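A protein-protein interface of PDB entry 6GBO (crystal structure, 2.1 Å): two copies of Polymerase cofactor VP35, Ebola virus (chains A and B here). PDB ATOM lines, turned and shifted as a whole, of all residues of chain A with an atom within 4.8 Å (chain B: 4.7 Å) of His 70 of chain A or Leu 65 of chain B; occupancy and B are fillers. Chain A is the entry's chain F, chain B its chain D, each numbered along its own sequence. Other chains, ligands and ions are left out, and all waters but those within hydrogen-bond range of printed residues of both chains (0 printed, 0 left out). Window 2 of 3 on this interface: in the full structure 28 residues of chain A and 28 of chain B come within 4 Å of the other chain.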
ATOM      1  N   LEU A  66     -13.923   5.829  22.187  1.00  0.00           N
ATOM      2  CA  LEU A  66     -14.706   6.079  23.403  1.00  0.00           C
ATOM      3  C   LEU A  66     -14.863   7.560  23.687  1.00  0.00           C
ATOM      4  O   LEU A  66     -15.933   8.004  24.108  1.00  0.00           O
ATOM      5  CB  LEU A  66     -14.088   5.385  24.618  1.00  0.00           C
ATOM      6  CG  LEU A  66     -14.128   3.859  24.596  1.00  0.00           C
ATOM      7  CD1 LEU A  66     -13.355   3.303  25.798  1.00  0.00           C
ATOM      8  CD2 LEU A  66     -15.554   3.334  24.584  1.00  0.00           C
ATOM      9  N   GLU A  67     -13.812   8.330  23.455  1.00  0.00           N
ATOM     10  CA  GLU A  67     -13.890   9.766  23.657  1.00  0.00           C
ATOM     11  C   GLU A  67     -14.872  10.389  22.668  1.00  0.00           C
ATOM     12  O   GLU A  67     -15.599  11.329  23.017  1.00  0.00           O
ATOM     13  CB  GLU A  67     -12.511  10.414  23.555  1.00  0.00           C
ATOM     14  CG  GLU A  67     -11.620  10.125  24.762  1.00  0.00           C
ATOM     15  CD  GLU A  67     -12.165  10.707  26.059  1.00  0.00           C
ATOM     16  OE1 GLU A  67     -12.622  11.865  26.043  1.00  0.00           O
ATOM     17  OE2 GLU A  67     -12.136  10.013  27.103  1.00  0.00           O
ATOM     18  N   HIS A  68     -14.911   9.857  21.447  1.00  0.00           N
ATOM     19  CA  HIS A  68     -15.880  10.306  20.459  1.00  0.00           C
ATOM     20  C   HIS A  68     -17.307  10.033  20.922  1.00  0.00           C
ATOM     21  O   HIS A  68     -18.153  10.923  20.859  1.00  0.00           O
ATOM     22  CB  HIS A  68     -15.628   9.645  19.109  1.00  0.00           C
ATOM     23  CG  HIS A  68     -16.742   9.836  18.131  1.00  0.00           C
ATOM     24  ND1 HIS A  68     -16.847  10.955  17.333  1.00  0.00           N
ATOM     25  CD2 HIS A  68     -17.806   9.055  17.828  1.00  0.00           C
ATOM     26  CE1 HIS A  68     -17.923  10.851  16.575  1.00  0.00           C
ATOM     27  NE2 HIS A  68     -18.522   9.708  16.855  1.00  0.00           N
ATOM     28  N   HIS A  69     -17.578   8.816  21.386  1.00  0.00           N
ATOM     29  CA  HIS A  69     -18.911   8.480  21.892  1.00  0.00           C
ATOM     30  C   HIS A  69     -19.323   9.360  23.073  1.00  0.00           C
ATOM     31  O   HIS A  69     -20.486   9.724  23.199  1.00  0.00           O
ATOM     32  CB  HIS A  69     -19.013   7.016  22.314  1.00  0.00           C
ATOM     33  CG  HIS A  69     -20.411   6.590  22.655  1.00  0.00           C
ATOM     34  ND1 HIS A  69     -21.206   5.878  21.780  1.00  0.00           N
ATOM     35  CD2 HIS A  69     -21.162   6.797  23.762  1.00  0.00           C
ATOM     36  CE1 HIS A  69     -22.384   5.657  22.339  1.00  0.00           C
ATOM     37  NE2 HIS A  69     -22.382   6.203  23.543  1.00  0.00           N
ATOM     38  N   HIS A  70     -18.365   9.674  23.941  1.00  0.00           N
ATOM     39  CA  HIS A  70     -18.599  10.564  25.070  1.00  0.00           C
ATOM     40  C   HIS A  70     -18.865  12.004  24.599  1.00  0.00           C
ATOM     41  O   HIS A  70     -19.741  12.682  25.129  1.00  0.00           O
ATOM     42  CB  HIS A  70     -17.395  10.511  26.029  1.00  0.00           C
ATOM     43  CG  HIS A  70     -17.569  11.326  27.276  1.00  0.00           C
ATOM     44  ND1 HIS A  70     -18.736  11.326  28.011  1.00  0.00           N
ATOM     45  CD2 HIS A  70     -16.717  12.156  27.924  1.00  0.00           C
ATOM     46  CE1 HIS A  70     -18.599  12.127  29.053  1.00  0.00           C
ATOM     47  NE2 HIS A  70     -17.382  12.643  29.023  1.00  0.00           N
ATOM     48  N   HIS A  71     -18.116  12.444  23.591  1.00  0.00           N
ATOM     49  CA  HIS A  71     -18.171  13.813  23.074  1.00  0.00           C
ATOM     50  C   HIS A  71     -19.309  14.072  22.064  1.00  0.00           C
ATOM     51  O   HIS A  71     -19.710  15.226  21.876  1.00  0.00           O
ATOM     52  CB  HIS A  71     -16.822  14.141  22.420  1.00  0.00           C
ATOM     53  CG  HIS A  71     -16.593  15.599  22.184  1.00  0.00           C
ATOM     54  ND1 HIS A  71     -16.018  16.424  23.129  1.00  0.00           N
ATOM     55  CD2 HIS A  71     -16.841  16.380  21.105  1.00  0.00           C
ATOM     56  CE1 HIS A  71     -15.934  17.652  22.646  1.00  0.00           C
ATOM     57  NE2 HIS A  71     -16.425  17.652  21.420  1.00  0.00           N
ATOM     58  N   HIS A  72     -19.806  13.020  21.405  1.00  0.00           N
ATOM     59  CA  HIS A  72     -20.841  13.159  20.363  1.00  0.00           C
ATOM     60  C   HIS A  72     -22.146  12.407  20.647  1.00  0.00           C
ATOM     61  O   HIS A  72     -23.108  12.539  19.892  1.00  0.00           O
ATOM     62  CB  HIS A  72     -20.288  12.723  18.999  1.00  0.00           C
ATOM     63  CG  HIS A  72     -19.291  13.678  18.411  1.00  0.00           C
ATOM     64  ND1 HIS A  72     -19.655  14.715  17.579  1.00  0.00           N
ATOM     65  CD2 HIS A  72     -17.944  13.752  18.536  1.00  0.00           C
ATOM     66  CE1 HIS A  72     -18.575  15.385  17.214  1.00  0.00           C
ATOM     67  NE2 HIS A  72     -17.524  14.822  17.783  1.00  0.00           N
ATOM     68  N   HIS A  73     -22.186  11.621  21.720  1.00  0.00           N
ATOM     69  CA  HIS A  73     -23.410  10.931  22.134  1.00  0.00           C
ATOM     70  C   HIS A  73     -23.592  11.084  23.640  1.00  0.00           C
ATOM     71  O   HIS A  73     -24.031  10.164  24.329  1.00  0.00           O
ATOM     72  CB  HIS A  73     -23.362   9.440  21.765  1.00  0.00           C
ATOM     73  CG  HIS A  73     -23.198   9.176  20.299  1.00  0.00           C
ATOM     74  ND1 HIS A  73     -21.994   9.322  19.644  1.00  0.00           N
ATOM     75  CD2 HIS A  73     -24.086   8.761  19.365  1.00  0.00           C
ATOM     76  CE1 HIS A  73     -22.148   9.016  18.368  1.00  0.00           C
ATOM     77  NE2 HIS A  73     -23.409   8.674  18.172  1.00  0.00           N
ATOM     78  OXT HIS A  73     -23.303  12.139  24.208  1.00  0.00           O
ATOM     79  N   LYS B  61     -14.020   2.277  31.218  1.00  0.00           N
ATOM     80  CA  LYS B  61     -14.518   3.384  30.400  1.00  0.00           C
ATOM     81  C   LYS B  61     -15.627   2.914  29.463  1.00  0.00           C
ATOM     82  O   LYS B  61     -16.652   3.580  29.326  1.00  0.00           O
ATOM     83  CB  LYS B  61     -13.363   3.965  29.607  1.00  0.00           C
ATOM     84  CG  LYS B  61     -13.534   5.381  29.105  1.00  0.00           C
ATOM     85  CD  LYS B  61     -12.152   6.016  29.135  1.00  0.00           C
ATOM     86  CE  LYS B  61     -12.092   7.347  28.434  1.00  0.00           C
ATOM     87  NZ  LYS B  61     -10.653   7.684  28.280  1.00  0.00           N
ATOM     88  N   TYR B  62     -15.427   1.761  28.837  1.00  0.00           N
ATOM     89  CA  TYR B  62     -16.467   1.125  28.032  1.00  0.00           C
ATOM     90  C   TYR B  62     -17.727   0.857  28.841  1.00  0.00           C
ATOM     91  O   TYR B  62     -18.841   1.110  28.384  1.00  0.00           O
ATOM     92  CB  TYR B  62     -15.970  -0.186  27.461  1.00  0.00           C
ATOM     93  CG  TYR B  62     -17.023  -0.994  26.740  1.00  0.00           C
ATOM     94  CD1 TYR B  62     -17.487  -0.610  25.486  1.00  0.00           C
ATOM     95  CD2 TYR B  62     -17.557  -2.152  27.313  1.00  0.00           C
ATOM     96  CE1 TYR B  62     -18.442  -1.360  24.818  1.00  0.00           C
ATOM     97  CE2 TYR B  62     -18.501  -2.912  26.651  1.00  0.00           C
ATOM     98  CZ  TYR B  62     -18.943  -2.514  25.405  1.00  0.00           C
ATOM     99  OH  TYR B  62     -19.902  -3.266  24.758  1.00  0.00           O
ATOM    100  N   ASP B  63     -17.519   0.315  30.035  1.00  0.00           N
ATOM    101  CA  ASP B  63     -18.595   0.052  30.966  1.00  0.00           C
ATOM    102  C   ASP B  63     -19.404   1.329  31.245  1.00  0.00           C
ATOM    103  O   ASP B  63     -20.608   1.314  31.157  1.00  0.00           O
ATOM    104  CB  ASP B  63     -18.025  -0.508  32.281  1.00  0.00           C
ATOM    105  CG  ASP B  63     -18.793  -1.699  32.803  1.00  0.00           C
ATOM    106  OD1 ASP B  63     -19.996  -1.852  32.515  1.00  0.00           O
ATOM    107  OD2 ASP B  63     -18.179  -2.493  33.526  1.00  0.00           O
ATOM    108  N   LEU B  64     -18.732   2.432  31.556  1.00  0.00           N
ATOM    109  CA  LEU B  64     -19.425   3.664  31.942  1.00  0.00           C
ATOM    110  C   LEU B  64     -20.160   4.356  30.804  1.00  0.00           C
ATOM    111  O   LEU B  64     -21.275   4.863  30.978  1.00  0.00           O
ATOM    112  CB  LEU B  64     -18.457   4.655  32.576  1.00  0.00           C
ATOM    113  CG  LEU B  64     -18.021   4.320  34.004  1.00  0.00           C
ATOM    114  CD1 LEU B  64     -17.094   5.409  34.513  1.00  0.00           C
ATOM    115  CD2 LEU B  64     -19.214   4.178  34.941  1.00  0.00           C
ATOM    116  N   LEU B  65     -19.525   4.373  29.645  1.00  0.00           N
ATOM    117  CA  LEU B  65     -19.987   5.178  28.533  1.00  0.00           C
ATOM    118  C   LEU B  65     -20.941   4.430  27.617  1.00  0.00           C
ATOM    119  O   LEU B  65     -21.807   5.047  27.007  1.00  0.00           O
ATOM    120  CB  LEU B  65     -18.785   5.703  27.735  1.00  0.00           C
ATOM    121  CG  LEU B  65     -17.840   6.615  28.530  1.00  0.00           C
ATOM    122  CD1 LEU B  65     -16.600   6.962  27.722  1.00  0.00           C
ATOM    123  CD2 LEU B  65     -18.571   7.878  28.967  1.00  0.00           C
ATOM    124  N   LEU B  66     -20.803   3.112  27.522  1.00  0.00           N
ATOM    125  CA  LEU B  66     -21.574   2.355  26.534  1.00  0.00           C
ATOM    126  C   LEU B  66     -22.565   1.349  27.112  1.00  0.00           C
ATOM    127  O   LEU B  66     -23.702   1.263  26.641  1.00  0.00           O
ATOM    128  CB  LEU B  66     -20.625   1.687  25.544  1.00  0.00           C
ATOM    129  CG  LEU B  66     -20.175   2.682  24.470  1.00  0.00           C
ATOM    130  CD1 LEU B  66     -18.766   2.409  23.981  1.00  0.00           C
ATOM    131  CD2 LEU B  66     -21.167   2.674  23.313  1.00  0.00           C
ATOM    132  N   GLU B  67     -22.156   0.604  28.131  1.00  0.00           N
ATOM    133  CA  GLU B  67     -23.053  -0.354  28.768  1.00  0.00           C
ATOM    134  C   GLU B  67     -24.293   0.323  29.387  1.00  0.00           C
ATOM    135  O   GLU B  67     -25.348  -0.305  29.482  1.00  0.00           O
ATOM    136  CB  GLU B  67     -22.288  -1.168  29.821  1.00  0.00           C
ATOM    137  CG  GLU B  67     -23.078  -2.293  30.486  1.00  0.00           C
ATOM    138  CD  GLU B  67     -23.534  -3.363  29.510  1.00  0.00           C
ATOM    139  OE1 GLU B  67     -22.847  -3.574  28.490  1.00  0.00           O
ATOM    140  OE2 GLU B  67     -24.577  -4.001  29.771  1.00  0.00           O
ATOM    141  N   HIS B  69     -24.931   4.435  29.415  1.00  0.00           N
ATOM    142  CA  HIS B  69     -25.364   5.698  28.814  1.00  0.00           C
ATOM    143  C   HIS B  69     -26.124   5.485  27.499  1.00  0.00           C
ATOM    144  O   HIS B  69     -25.864   4.533  26.761  1.00  0.00           O
ATOM    145  CB  HIS B  69     -24.161   6.614  28.580  1.00  0.00           C
ATOM    146  CG  HIS B  69     -24.533   8.027  28.256  1.00  0.00           C
ATOM    147  ND1 HIS B  69     -24.977   8.918  29.210  1.00  0.00           N
ATOM    148  CD2 HIS B  69     -24.529   8.703  27.083  1.00  0.00           C
ATOM    149  CE1 HIS B  69     -25.232  10.082  28.639  1.00  0.00           C
ATOM    150  NE2 HIS B  69     -24.967   9.979  27.349  1.00  0.00           N
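The side-chain carboxylate (OE2) of Glu 67 of chain A is in salt-bridge range of the side-chain amino group (NZ) of Lys 61 of chain B. O of His 73 of chain A sits close to NE2 of His 69 of chain B (3.2 Å).
N of Glu 67 of chain B is in hydrogen-bond range of O of Tyr 62 of chain B (3.4 Å).
Lys 61 of chain B touches Leu 66 of chain A. CD1 of Leu 66 of chain A touches N of Tyr 62 of chain B (3.99 Å). O of Leu 66 of chain A touches CD1 of Leu 65 of chain B, at 3.8 Å. Leu 66 of chain B touches Leu 66 of chain A (CD1 to CD2, 3.4 Å). NE2 of His 69 of chain A touches O of Leu 65 of chain B (3.7 Å). His 69 of chain A touches Leu 66 of chain B. Leu 65 of chain B touches His 70 of chain A (CD2 to ND1, 3.6 Å).
His 70 of chain A touches one residue of chain B. Of chain A, only Leu 66, His 69 and His 70 come within 4 Å of Leu 65 of chain B. Of the printed residues of chain B, His 69 of chain A touches Leu 65 and Leu 66. Printed residues of chain B within 4 Å of Leu 66 of chain A: Lys 61, Tyr 62, Leu 65 and Leu 66. Glu 67 of chain B touches none of the printed residues of chain A. His 72 of chain A touches none of the printed residues of chain B. The nearest printed residue of chain A that does not touch Leu 65 of chain B is Glu 67 of chain A (5.3 Å).
Printed residues of chain A that touch a printed residue of chain B: Leu 66, Glu 67, His 69, His 70 and His 73. Hydrophobic or aromatic side chains of chain B within 4 Å of the printed part of chain A: Leu 65, Leu 66 and His 69. Among the printed residues, 9 pairs touch across the chains.
Leu 66 of chain A touches its own counterpart, Leu 66 of chain B. His 69 of chain A touches Leu 66 of chain B, but with the chains exchanged Leu 66 of chain A does not touch His 69 of chain B (9.1 Å). 3 positions are printed for both chains. Of the 9 pairs that touch across the chains among the printed residues, 1 has its exchanged pair printed and touching as well.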
